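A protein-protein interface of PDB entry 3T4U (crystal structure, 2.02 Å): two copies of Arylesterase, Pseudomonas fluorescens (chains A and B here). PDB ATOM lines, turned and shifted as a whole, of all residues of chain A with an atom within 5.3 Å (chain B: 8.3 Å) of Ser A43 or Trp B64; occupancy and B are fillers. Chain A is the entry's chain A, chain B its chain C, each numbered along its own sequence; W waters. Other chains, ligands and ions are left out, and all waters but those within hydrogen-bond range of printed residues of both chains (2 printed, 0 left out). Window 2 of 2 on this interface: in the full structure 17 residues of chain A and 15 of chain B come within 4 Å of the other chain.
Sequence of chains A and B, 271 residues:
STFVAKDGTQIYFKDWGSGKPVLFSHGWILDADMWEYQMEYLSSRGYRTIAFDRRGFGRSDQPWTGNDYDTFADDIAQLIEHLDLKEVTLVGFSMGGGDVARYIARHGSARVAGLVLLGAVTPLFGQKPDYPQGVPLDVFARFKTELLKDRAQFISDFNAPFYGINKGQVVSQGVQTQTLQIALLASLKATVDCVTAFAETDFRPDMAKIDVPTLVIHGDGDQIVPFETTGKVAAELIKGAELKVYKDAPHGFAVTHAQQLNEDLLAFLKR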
ATOM      1  N   ASP A  15      17.549 -19.305  19.109  1.00  0.00           N
ATOM      2  CA  ASP A  15      18.115 -20.585  18.730  1.00  0.00           C
ATOM      3  C   ASP A  15      18.829 -21.048  19.990  1.00  0.00           C
ATOM      4  O   ASP A  15      19.881 -20.507  20.361  1.00  0.00           O
ATOM      5  CB  ASP A  15      19.079 -20.433  17.541  1.00  0.00           C
ATOM      6  CG  ASP A  15      19.719 -21.771  17.116  1.00  0.00           C
ATOM      7  OD1 ASP A  15      19.423 -22.816  17.723  1.00  0.00           O
ATOM      8  OD2 ASP A  15      20.544 -21.765  16.173  1.00  0.00           O
ATOM      9  N   TRP A  16      18.214 -22.014  20.665  1.00  0.00           N
ATOM     10  CA  TRP A  16      18.632 -22.411  21.995  1.00  0.00           C
ATOM     11  C   TRP A  16      18.994 -23.903  22.010  1.00  0.00           C
ATOM     12  O   TRP A  16      18.307 -24.713  21.392  1.00  0.00           O
ATOM     13  CB  TRP A  16      17.459 -22.228  22.962  1.00  0.00           C
ATOM     14  CG  TRP A  16      17.151 -20.830  23.391  1.00  0.00           C
ATOM     15  CD1 TRP A  16      17.829 -19.676  23.071  1.00  0.00           C
ATOM     16  CD2 TRP A  16      16.104 -20.451  24.278  1.00  0.00           C
ATOM     17  NE1 TRP A  16      17.243 -18.595  23.710  1.00  0.00           N
ATOM     18  CE2 TRP A  16      16.190 -19.051  24.458  1.00  0.00           C
ATOM     19  CE3 TRP A  16      15.100 -21.164  24.949  1.00  0.00           C
ATOM     20  CZ2 TRP A  16      15.289 -18.335  25.279  1.00  0.00           C
ATOM     21  CZ3 TRP A  16      14.191 -20.459  25.752  1.00  0.00           C
ATOM     22  CH2 TRP A  16      14.318 -19.052  25.926  1.00  0.00           C
ATOM     23  N   GLY A  17      20.031 -24.251  22.770  1.00  0.00           N
ATOM     24  CA  GLY A  17      20.358 -25.646  23.046  1.00  0.00           C
ATOM     25  C   GLY A  17      21.135 -26.308  21.932  1.00  0.00           C
ATOM     26  O   GLY A  17      21.548 -25.660  20.977  1.00  0.00           O
ATOM     27  N   GLN A  38       8.040 -24.169  26.504  1.00  0.00           N
ATOM     28  CA  GLN A  38       8.292 -25.410  25.755  1.00  0.00           C
ATOM     29  C   GLN A  38       9.752 -25.495  25.325  1.00  0.00           C
ATOM     30  O   GLN A  38      10.379 -26.579  25.400  1.00  0.00           O
ATOM     31  CB  GLN A  38       7.361 -25.531  24.539  1.00  0.00           C
ATOM     32  CG  GLN A  38       5.953 -25.956  24.900  1.00  0.00           C
ATOM     33  CD  GLN A  38       5.152 -24.833  25.552  1.00  0.00           C
ATOM     34  OE1 GLN A  38       5.080 -23.727  25.014  1.00  0.00           O
ATOM     35  NE2 GLN A  38       4.562 -25.103  26.719  1.00  0.00           N
ATOM     36  N   MET A  39      10.304 -24.347  24.928  1.00  0.00           N
ATOM     37  CA  MET A  39      11.727 -24.244  24.530  1.00  0.00           C
ATOM     38  C   MET A  39      12.676 -24.570  25.680  1.00  0.00           C
ATOM     39  O   MET A  39      13.616 -25.360  25.508  1.00  0.00           O
ATOM     40  CB  MET A  39      12.053 -22.849  23.978  1.00  0.00           C
ATOM     41  CG  MET A  39      11.366 -22.589  22.640  1.00  0.00           C
ATOM     42  SD  MET A  39      11.759 -20.979  21.982  1.00  0.00           S
ATOM     43  CE  MET A  39      13.491 -21.158  21.474  1.00  0.00           C
ATOM     44  N   GLU A  40      12.438 -23.953  26.842  1.00  0.00           N
ATOM     45  CA  GLU A  40      13.251 -24.240  28.013  1.00  0.00           C
ATOM     46  C   GLU A  40      13.120 -25.712  28.393  1.00  0.00           C
ATOM     47  O   GLU A  40      14.109 -26.362  28.681  1.00  0.00           O
ATOM     48  CB  GLU A  40      12.868 -23.347  29.194  1.00  0.00           C
ATOM     49  CG  GLU A  40      13.804 -23.488  30.403  1.00  0.00           C
ATOM     50  CD  GLU A  40      13.497 -24.701  31.322  1.00  0.00           C
ATOM     51  OE1 GLU A  40      14.385 -25.056  32.106  1.00  0.00           O
ATOM     52  OE2 GLU A  40      12.401 -25.288  31.278  1.00  0.00           O
ATOM     53  N   TYR A  41      11.897 -26.224  28.363  1.00  0.00           N
ATOM     54  CA  TYR A  41      11.627 -27.592  28.740  1.00  0.00           C
ATOM     55  C   TYR A  41      12.406 -28.581  27.857  1.00  0.00           C
ATOM     56  O   TYR A  41      13.114 -29.458  28.378  1.00  0.00           O
ATOM     57  CB  TYR A  41      10.124 -27.860  28.714  1.00  0.00           C
ATOM     58  CG  TYR A  41       9.742 -29.249  29.157  1.00  0.00           C
ATOM     59  CD1 TYR A  41       9.470 -29.534  30.503  1.00  0.00           C
ATOM     60  CD2 TYR A  41       9.668 -30.293  28.229  1.00  0.00           C
ATOM     61  CE1 TYR A  41       9.125 -30.838  30.910  1.00  0.00           C
ATOM     62  CE2 TYR A  41       9.320 -31.572  28.620  1.00  0.00           C
ATOM     63  CZ  TYR A  41       9.058 -31.841  29.956  1.00  0.00           C
ATOM     64  OH  TYR A  41       8.704 -33.126  30.292  1.00  0.00           O
ATOM     65  N   LEU A  42      12.317 -28.410  26.537  1.00  0.00           N
ATOM     66  CA  LEU A  42      12.983 -29.318  25.596  1.00  0.00           C
ATOM     67  C   LEU A  42      14.476 -29.092  25.497  1.00  0.00           C
ATOM     68  O   LEU A  42      15.253 -30.069  25.416  1.00  0.00           O
ATOM     69  CB  LEU A  42      12.341 -29.220  24.219  1.00  0.00           C
ATOM     70  CG  LEU A  42      10.878 -29.685  24.218  1.00  0.00           C
ATOM     71  CD1 LEU A  42      10.233 -29.373  22.854  1.00  0.00           C
ATOM     72  CD2 LEU A  42      10.732 -31.200  24.553  1.00  0.00           C
ATOM     73  N   SER A  43      14.903 -27.828  25.492  1.00  0.00           N
ATOM     74  CA  SER A  43      16.334 -27.567  25.448  1.00  0.00           C
ATOM     75  C   SER A  43      17.072 -28.010  26.697  1.00  0.00           C
ATOM     76  O   SER A  43      18.260 -28.261  26.614  1.00  0.00           O
ATOM     77  CB  SER A  43      16.682 -26.116  25.060  1.00  0.00           C
ATOM     78  OG  SER A  43      16.466 -25.966  23.670  1.00  0.00           O
ATOM     79  N   SER A  44      16.381 -28.126  27.834  1.00  0.00           N
ATOM     80  CA  SER A  44      16.983 -28.656  29.064  1.00  0.00           C
ATOM     81  C   SER A  44      17.064 -30.187  29.024  1.00  0.00           C
ATOM     82  O   SER A  44      17.700 -30.801  29.872  1.00  0.00           O
ATOM     83  CB  SER A  44      16.169 -28.247  30.295  1.00  0.00           C
ATOM     84  OG  SER A  44      16.424 -26.911  30.657  1.00  0.00           O
ATOM     85  N   ARG A  45      16.383 -30.789  28.048  1.00  0.00           N
ATOM     86  CA  ARG A  45      16.315 -32.246  27.902  1.00  0.00           C
ATOM     87  C   ARG A  45      16.892 -32.719  26.573  1.00  0.00           C
ATOM     88  O   ARG A  45      16.408 -33.706  26.013  1.00  0.00           O
ATOM     89  CB  ARG A  45      14.872 -32.725  28.061  1.00  0.00           C
ATOM     90  CG  ARG A  45      14.343 -32.524  29.470  1.00  0.00           C
ATOM     91  CD  ARG A  45      12.835 -32.570  29.545  1.00  0.00           C
ATOM     92  NE  ARG A  45      12.388 -32.561  30.937  1.00  0.00           N
ATOM     93  CZ  ARG A  45      12.342 -31.479  31.717  1.00  0.00           C
ATOM     94  NH1 ARG A  45      12.681 -30.260  31.261  1.00  0.00           N
ATOM     95  NH2 ARG A  45      11.924 -31.607  32.961  1.00  0.00           N
ATOM     96  N   GLY A  46      17.880 -31.988  26.061  1.00  0.00           N
ATOM     97  CA  GLY A  46      18.777 -32.480  25.000  1.00  0.00           C
ATOM     98  C   GLY A  46      18.326 -32.161  23.588  1.00  0.00           C
ATOM     99  O   GLY A  46      18.740 -32.834  22.621  1.00  0.00           O
ATOM    100  N   TYR A  47      17.460 -31.148  23.459  1.00  0.00           N
ATOM    101  CA  TYR A  47      17.019 -30.697  22.129  1.00  0.00           C
ATOM    102  C   TYR A  47      17.454 -29.290  21.817  1.00  0.00           C
ATOM    103  O   TYR A  47      17.698 -28.487  22.724  1.00  0.00           O
ATOM    104  CB  TYR A  47      15.508 -30.829  21.998  1.00  0.00           C
ATOM    105  CG  TYR A  47      15.098 -32.284  22.007  1.00  0.00           C
ATOM    106  CD1 TYR A  47      15.194 -33.052  20.843  1.00  0.00           C
ATOM    107  CD2 TYR A  47      14.651 -32.899  23.175  1.00  0.00           C
ATOM    108  CE1 TYR A  47      14.830 -34.401  20.837  1.00  0.00           C
ATOM    109  CE2 TYR A  47      14.285 -34.243  23.184  1.00  0.00           C
ATOM    110  CZ  TYR A  47      14.387 -34.983  22.006  1.00  0.00           C
ATOM    111  OH  TYR A  47      14.036 -36.302  21.984  1.00  0.00           O
ATOM    112  N   ARG A  48      17.566 -29.000  20.522  1.00  0.00           N
ATOM    113  CA  ARG A  48      17.810 -27.653  20.065  1.00  0.00           C
ATOM    114  C   ARG A  48      16.442 -27.089  19.722  1.00  0.00           C
ATOM    115  O   ARG A  48      15.686 -27.744  19.027  1.00  0.00           O
ATOM    116  CB  ARG A  48      18.737 -27.670  18.830  1.00  0.00           C
ATOM    117  CG  ARG A  48      19.022 -26.293  18.249  1.00  0.00           C
ATOM    118  CD  ARG A  48      20.005 -26.435  17.081  1.00  0.00           C
ATOM    119  NE  ARG A  48      20.367 -25.161  16.479  1.00  0.00           N
ATOM    120  CZ  ARG A  48      21.013 -25.053  15.313  1.00  0.00           C
ATOM    121  NH1 ARG A  48      21.370 -26.159  14.641  1.00  0.00           N
ATOM    122  NH2 ARG A  48      21.307 -23.855  14.813  1.00  0.00           N
ATOM    123  N   THR A  49      16.099 -25.907  20.254  1.00  0.00           N
ATOM    124  CA  THR A  49      14.788 -25.301  20.006  1.00  0.00           C
ATOM    125  C   THR A  49      14.985 -23.943  19.309  1.00  0.00           C
ATOM    126  O   THR A  49      15.888 -23.173  19.659  1.00  0.00           O
ATOM    127  CB  THR A  49      13.887 -25.188  21.305  1.00  0.00           C
ATOM    128  OG1 THR A  49      14.542 -24.382  22.298  1.00  0.00           O
ATOM    129  CG2 THR A  49      13.591 -26.562  21.861  1.00  0.00           C
ATOM    130  N   ASP B   7      30.795 -14.822  22.083  1.00  0.00           N
ATOM    131  CA  ASP B   7      30.001 -15.923  21.567  1.00  0.00           C
ATOM    132  C   ASP B   7      28.981 -15.482  20.507  1.00  0.00           C
ATOM    133  O   ASP B   7      28.189 -16.284  20.073  1.00  0.00           O
ATOM    134  CB  ASP B   7      29.336 -16.728  22.700  1.00  0.00           C
ATOM    135  CG  ASP B   7      28.168 -15.973  23.379  1.00  0.00           C
ATOM    136  OD1 ASP B   7      27.517 -16.540  24.285  1.00  0.00           O
ATOM    137  OD2 ASP B   7      27.908 -14.825  23.016  1.00  0.00           O
ATOM    138  N   THR B   9      26.706 -12.941  21.089  1.00  0.00           N
ATOM    139  CA  THR B   9      25.571 -12.280  21.731  1.00  0.00           C
ATOM    140  C   THR B   9      25.631 -10.757  21.562  1.00  0.00           C
ATOM    141  O   THR B   9      26.598 -10.108  21.962  1.00  0.00           O
ATOM    142  CB  THR B   9      25.501 -12.626  23.239  1.00  0.00           C
ATOM    143  OG1 THR B   9      25.312 -14.038  23.387  1.00  0.00           O
ATOM    144  CG2 THR B   9      24.316 -11.885  23.893  1.00  0.00           C
ATOM    145  N   ARG B  55      23.165  -9.784  29.067  1.00  0.00           N
ATOM    146  CA  ARG B  55      22.694 -10.858  28.186  1.00  0.00           C
ATOM    147  C   ARG B  55      21.416 -11.532  28.725  1.00  0.00           C
ATOM    148  O   ARG B  55      21.330 -11.834  29.918  1.00  0.00           O
ATOM    149  CB  ARG B  55      23.782 -11.910  27.916  1.00  0.00           C
ATOM    150  CG  ARG B  55      24.303 -12.697  29.155  1.00  0.00           C
ATOM    151  CD  ARG B  55      25.241 -13.856  28.685  1.00  0.00           C
ATOM    152  NE  ARG B  55      26.399 -13.366  27.905  1.00  0.00           N
ATOM    153  CZ  ARG B  55      26.954 -14.046  26.893  1.00  0.00           C
ATOM    154  NH1 ARG B  55      27.997 -13.549  26.222  1.00  0.00           N
ATOM    155  NH2 ARG B  55      26.452 -15.228  26.540  1.00  0.00           N
ATOM    156  N   GLY B  56      20.445 -11.742  27.832  1.00  0.00           N
ATOM    157  CA  GLY B  56      19.135 -12.284  28.184  1.00  0.00           C
ATOM    158  C   GLY B  56      18.116 -11.288  28.740  1.00  0.00           C
ATOM    159  O   GLY B  56      17.000 -11.677  29.052  1.00  0.00           O
ATOM    160  N   ASP B  61      20.312  -9.638  23.069  1.00  0.00           N
ATOM    161  CA  ASP B  61      20.030 -11.030  22.626  1.00  0.00           C
ATOM    162  C   ASP B  61      19.865 -11.965  23.826  1.00  0.00           C
ATOM    163  O   ASP B  61      20.277 -11.632  24.937  1.00  0.00           O
ATOM    164  CB  ASP B  61      21.188 -11.567  21.751  1.00  0.00           C
ATOM    165  CG  ASP B  61      21.177 -10.999  20.330  1.00  0.00           C
ATOM    166  OD1 ASP B  61      20.254 -10.238  19.965  1.00  0.00           O
ATOM    167  OD2 ASP B  61      22.114 -11.309  19.568  1.00  0.00           O
ATOM    168  N   GLN B  62      19.256 -13.127  23.587  1.00  0.00           N
ATOM    169  CA  GLN B  62      18.975 -14.085  24.633  1.00  0.00           C
ATOM    170  C   GLN B  62      19.676 -15.451  24.438  1.00  0.00           C
ATOM    171  O   GLN B  62      19.018 -16.430  24.115  1.00  0.00           O
ATOM    172  CB  GLN B  62      17.462 -14.288  24.774  1.00  0.00           C
ATOM    173  CG  GLN B  62      16.608 -12.981  24.736  1.00  0.00           C
ATOM    174  CD  GLN B  62      15.111 -13.246  24.978  1.00  0.00           C
ATOM    175  OE1 GLN B  62      14.642 -14.398  24.950  1.00  0.00           O
ATOM    176  NE2 GLN B  62      14.361 -12.177  25.253  1.00  0.00           N
ATOM    177  N   PRO B  63      21.001 -15.526  24.681  1.00  0.00           N
ATOM    178  CA  PRO B  63      21.664 -16.813  24.526  1.00  0.00           C
ATOM    179  C   PRO B  63      21.208 -17.876  25.536  1.00  0.00           C
ATOM    180  O   PRO B  63      20.922 -17.586  26.728  1.00  0.00           O
ATOM    181  CB  PRO B  63      23.149 -16.475  24.729  1.00  0.00           C
ATOM    182  CG  PRO B  63      23.137 -15.231  25.602  1.00  0.00           C
ATOM    183  CD  PRO B  63      21.954 -14.460  25.040  1.00  0.00           C
ATOM    184  N   TRP B  64      21.180 -19.117  25.055  1.00  0.00           N
ATOM    185  CA  TRP B  64      20.935 -20.281  25.908  1.00  0.00           C
ATOM    186  C   TRP B  64      22.119 -20.484  26.851  1.00  0.00           C
ATOM    187  O   TRP B  64      21.920 -20.817  28.020  1.00  0.00           O
ATOM    188  CB  TRP B  64      20.719 -21.544  25.057  1.00  0.00           C
ATOM    189  CG  TRP B  64      20.504 -22.813  25.888  1.00  0.00           C
ATOM    190  CD1 TRP B  64      21.427 -23.818  26.136  1.00  0.00           C
ATOM    191  CD2 TRP B  64      19.315 -23.190  26.576  1.00  0.00           C
ATOM    192  NE1 TRP B  64      20.862 -24.789  26.936  1.00  0.00           N
ATOM    193  CE2 TRP B  64      19.569 -24.434  27.215  1.00  0.00           C
ATOM    194  CE3 TRP B  64      18.050 -22.597  26.723  1.00  0.00           C
ATOM    195  CZ2 TRP B  64      18.603 -25.088  27.984  1.00  0.00           C
ATOM    196  CZ3 TRP B  64      17.095 -23.254  27.466  1.00  0.00           C
ATOM    197  CH2 TRP B  64      17.372 -24.487  28.095  1.00  0.00           C
ATOM    198  N   THR B  65      23.340 -20.261  26.342  1.00  0.00           N
ATOM    199  CA  THR B  65      24.565 -20.496  27.103  1.00  0.00           C
ATOM    200  C   THR B  65      25.192 -19.197  27.624  1.00  0.00           C
ATOM    201  O   THR B  65      24.854 -18.082  27.199  1.00  0.00           O
ATOM    202  CB  THR B  65      25.666 -21.258  26.270  1.00  0.00           C
ATOM    203  OG1 THR B  65      26.120 -20.392  25.236  1.00  0.00           O
ATOM    204  CG2 THR B  65      25.132 -22.577  25.650  1.00  0.00           C
ATOM    205  N   GLY B  66      26.086 -19.356  28.586  1.00  0.00           N
ATOM    206  CA  GLY B  66      26.862 -18.234  29.086  1.00  0.00           C
ATOM    207  C   GLY B  66      26.135 -17.378  30.114  1.00  0.00           C
ATOM    208  O   GLY B  66      26.589 -16.290  30.415  1.00  0.00           O
ATOM    209  N   ASN B  67      25.031 -17.868  30.672  1.00  0.00           N
ATOM    210  CA  ASN B  67      24.313 -17.127  31.735  1.00  0.00           C
ATOM    211  C   ASN B  67      24.933 -17.390  33.136  1.00  0.00           C
ATOM    212  O   ASN B  67      24.297 -17.981  34.027  1.00  0.00           O
ATOM    213  CB  ASN B  67      22.823 -17.460  31.694  1.00  0.00           C
ATOM    214  CG  ASN B  67      22.176 -17.076  30.343  1.00  0.00           C
ATOM    215  OD1 ASN B  67      22.331 -15.953  29.869  1.00  0.00           O
ATOM    216  ND2 ASN B  67      21.479 -18.010  29.732  1.00  0.00           N
ATOM    217  N   ASP B  68      26.181 -16.961  33.308  1.00  0.00           N
ATOM    218  CA  ASP B  68      26.935 -17.232  34.532  1.00  0.00           C
ATOM    219  C   ASP B  68      27.839 -16.056  34.772  1.00  0.00           C
ATOM    220  O   ASP B  68      28.015 -15.234  33.882  1.00  0.00           O
ATOM    221  CB  ASP B  68      27.748 -18.524  34.413  1.00  0.00           C
ATOM    222  CG  ASP B  68      28.724 -18.489  33.238  1.00  0.00           C
ATOM    223  OD1 ASP B  68      29.775 -17.864  33.336  1.00  0.00           O
ATOM    224  OD2 ASP B  68      28.413 -19.090  32.212  1.00  0.00           O
ATOM    225  N   SER B 187      14.599 -12.974  28.673  1.00  0.00           N
ATOM    226  CA  SER B 187      14.497 -14.395  28.423  1.00  0.00           C
ATOM    227  C   SER B 187      14.045 -15.152  29.672  1.00  0.00           C
ATOM    228  O   SER B 187      14.560 -14.920  30.764  1.00  0.00           O
ATOM    229  CB  SER B 187      15.880 -14.933  28.021  1.00  0.00           C
ATOM    230  OG  SER B 187      15.889 -16.356  28.082  1.00  0.00           O
ATOM    231  N   LEU B 188      13.120 -16.092  29.505  1.00  0.00           N
ATOM    232  CA  LEU B 188      12.783 -17.006  30.614  1.00  0.00           C
ATOM    233  C   LEU B 188      14.031 -17.738  31.068  1.00  0.00           C
ATOM    234  O   LEU B 188      14.283 -17.886  32.269  1.00  0.00           O
ATOM    235  CB  LEU B 188      11.734 -18.047  30.197  1.00  0.00           C
ATOM    236  CG  LEU B 188      11.512 -19.205  31.168  1.00  0.00           C
ATOM    237  CD1 LEU B 188      10.932 -18.696  32.530  1.00  0.00           C
ATOM    238  CD2 LEU B 188      10.545 -20.227  30.552  1.00  0.00           C
ATOM    239  N   LYS B 189      14.817 -18.191  30.090  1.00  0.00           N
ATOM    240  CA  LYS B 189      16.027 -18.973  30.370  1.00  0.00           C
ATOM    241  C   LYS B 189      17.019 -18.145  31.193  1.00  0.00           C
ATOM    242  O   LYS B 189      17.569 -18.635  32.187  1.00  0.00           O
ATOM    243  CB  LYS B 189      16.668 -19.472  29.052  1.00  0.00           C
ATOM    244  CG  LYS B 189      18.054 -20.124  29.228  1.00  0.00           C
ATOM    245  CD  LYS B 189      18.060 -21.300  30.236  1.00  0.00           C
ATOM    246  CE  LYS B 189      19.389 -22.085  30.130  1.00  0.00           C
ATOM    247  NZ  LYS B 189      19.491 -23.141  31.197  1.00  0.00           N
ATOM    248  N   ALA B 190      17.265 -16.900  30.780  1.00  0.00           N
ATOM    249  CA  ALA B 190      18.230 -16.088  31.492  1.00  0.00           C
ATOM    250  C   ALA B 190      17.683 -15.750  32.884  1.00  0.00           C
ATOM    251  O   ALA B 190      18.446 -15.724  33.855  1.00  0.00           O
ATOM    252  CB  ALA B 190      18.564 -14.799  30.728  1.00  0.00           C
ATOM    253  N   ASP B 193      18.288 -18.920  34.993  1.00  0.00           N
ATOM    254  CA  ASP B 193      19.750 -19.141  35.096  1.00  0.00           C
ATOM    255  C   ASP B 193      20.387 -18.145  36.050  1.00  0.00           C
ATOM    256  O   ASP B 193      21.311 -18.485  36.783  1.00  0.00           O
ATOM    257  CB  ASP B 193      20.443 -19.000  33.741  1.00  0.00           C
ATOM    258  CG  ASP B 193      20.543 -20.322  32.979  1.00  0.00           C
ATOM    259  OD1 ASP B 193      19.963 -21.318  33.428  1.00  0.00           O
ATOM    260  OD2 ASP B 193      21.200 -20.361  31.909  1.00  0.00           O
HETATM  261  O   HOH W   1      21.657 -19.725  22.206  1.00  0.00           O
HETATM  262  O   HOH W   2      17.070 -24.259  32.283  1.00  0.00           O
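NE1 of Trp A16 is in hydrogen-bond range of O of Gln B62, at 2.8 Å.
OG of Ser A43 lies close to O of Met A39 (3.4 Å). The side-chain hydroxyl (OG) of Ser A43 lies within hydrogen-bond range of the side-chain hydroxyl (OG1) of Thr A49 (2.8 Å). The backbone carbonyl oxygen (O) of Gly B56 lies within hydrogen-bond range of the backbone NH (N) of Ser B187. The side-chain hydroxyl of Ser B187 is in hydrogen-bond range of the backbone NH of Lys B189. OG of Ser B187 sits at hydrogen-bond distance from N of Ala B190, 3.1 Å away. NZ of Lys B189 lies within salt-bridge range of OD1 of Asp B193 (2.9 Å).
Among the printed residues, pairs that only touch across the chains: Gly A17 with Trp B64, Ser A43 with Trp B64, Trp A16 with Ser B187, Ser A44 with Trp B64, Trp A16 with Trp B64, Glu A40 with Trp B64 and Trp A16 with Lys B189.
Printed residues of chain B within 4 Å of Glu A40: Trp B64. Ser A43 touches one residue of chain B. Of the printed residues of chain A, Gln B62 touches Trp A16. Of the printed residues of chain A, Lys B189 touches Trp A16. The nearest residue of chain B that does not touch Ser A43 is Lys B189 (7.0 Å). The nearest printed residue of chain A that does not touch Lys B189 is Glu A40 (4.8 Å).
Of the 17 printed residues of chain B, 4 touch a printed residue of chain A. Of the 15 printed residues of chain A, 5 touch a printed residue of chain B. Among the printed residues, 8 pairs touch across the chains. Among the printed residues, no Asp or Glu carboxylate lies within 4 Å of a Lys or Arg side-chain nitrogen of the other chain.
No position is printed for both chains. Of the 8 pairs that touch across the chains among the printed residues, none has its exchanged pair printed and touching as well.
Water W1 bridges the backbone carbonyl oxygen of Asp A15 (2.7 Å) and the backbone NH of Trp B64 (3.0 Å). Water W2 lies within hydrogen-bond range of the side-chain carboxylate (OE1) of Glu A40, the side-chain amino group (NZ) of Lys B189 and the side-chain hydroxyl (OG) of Ser A44.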
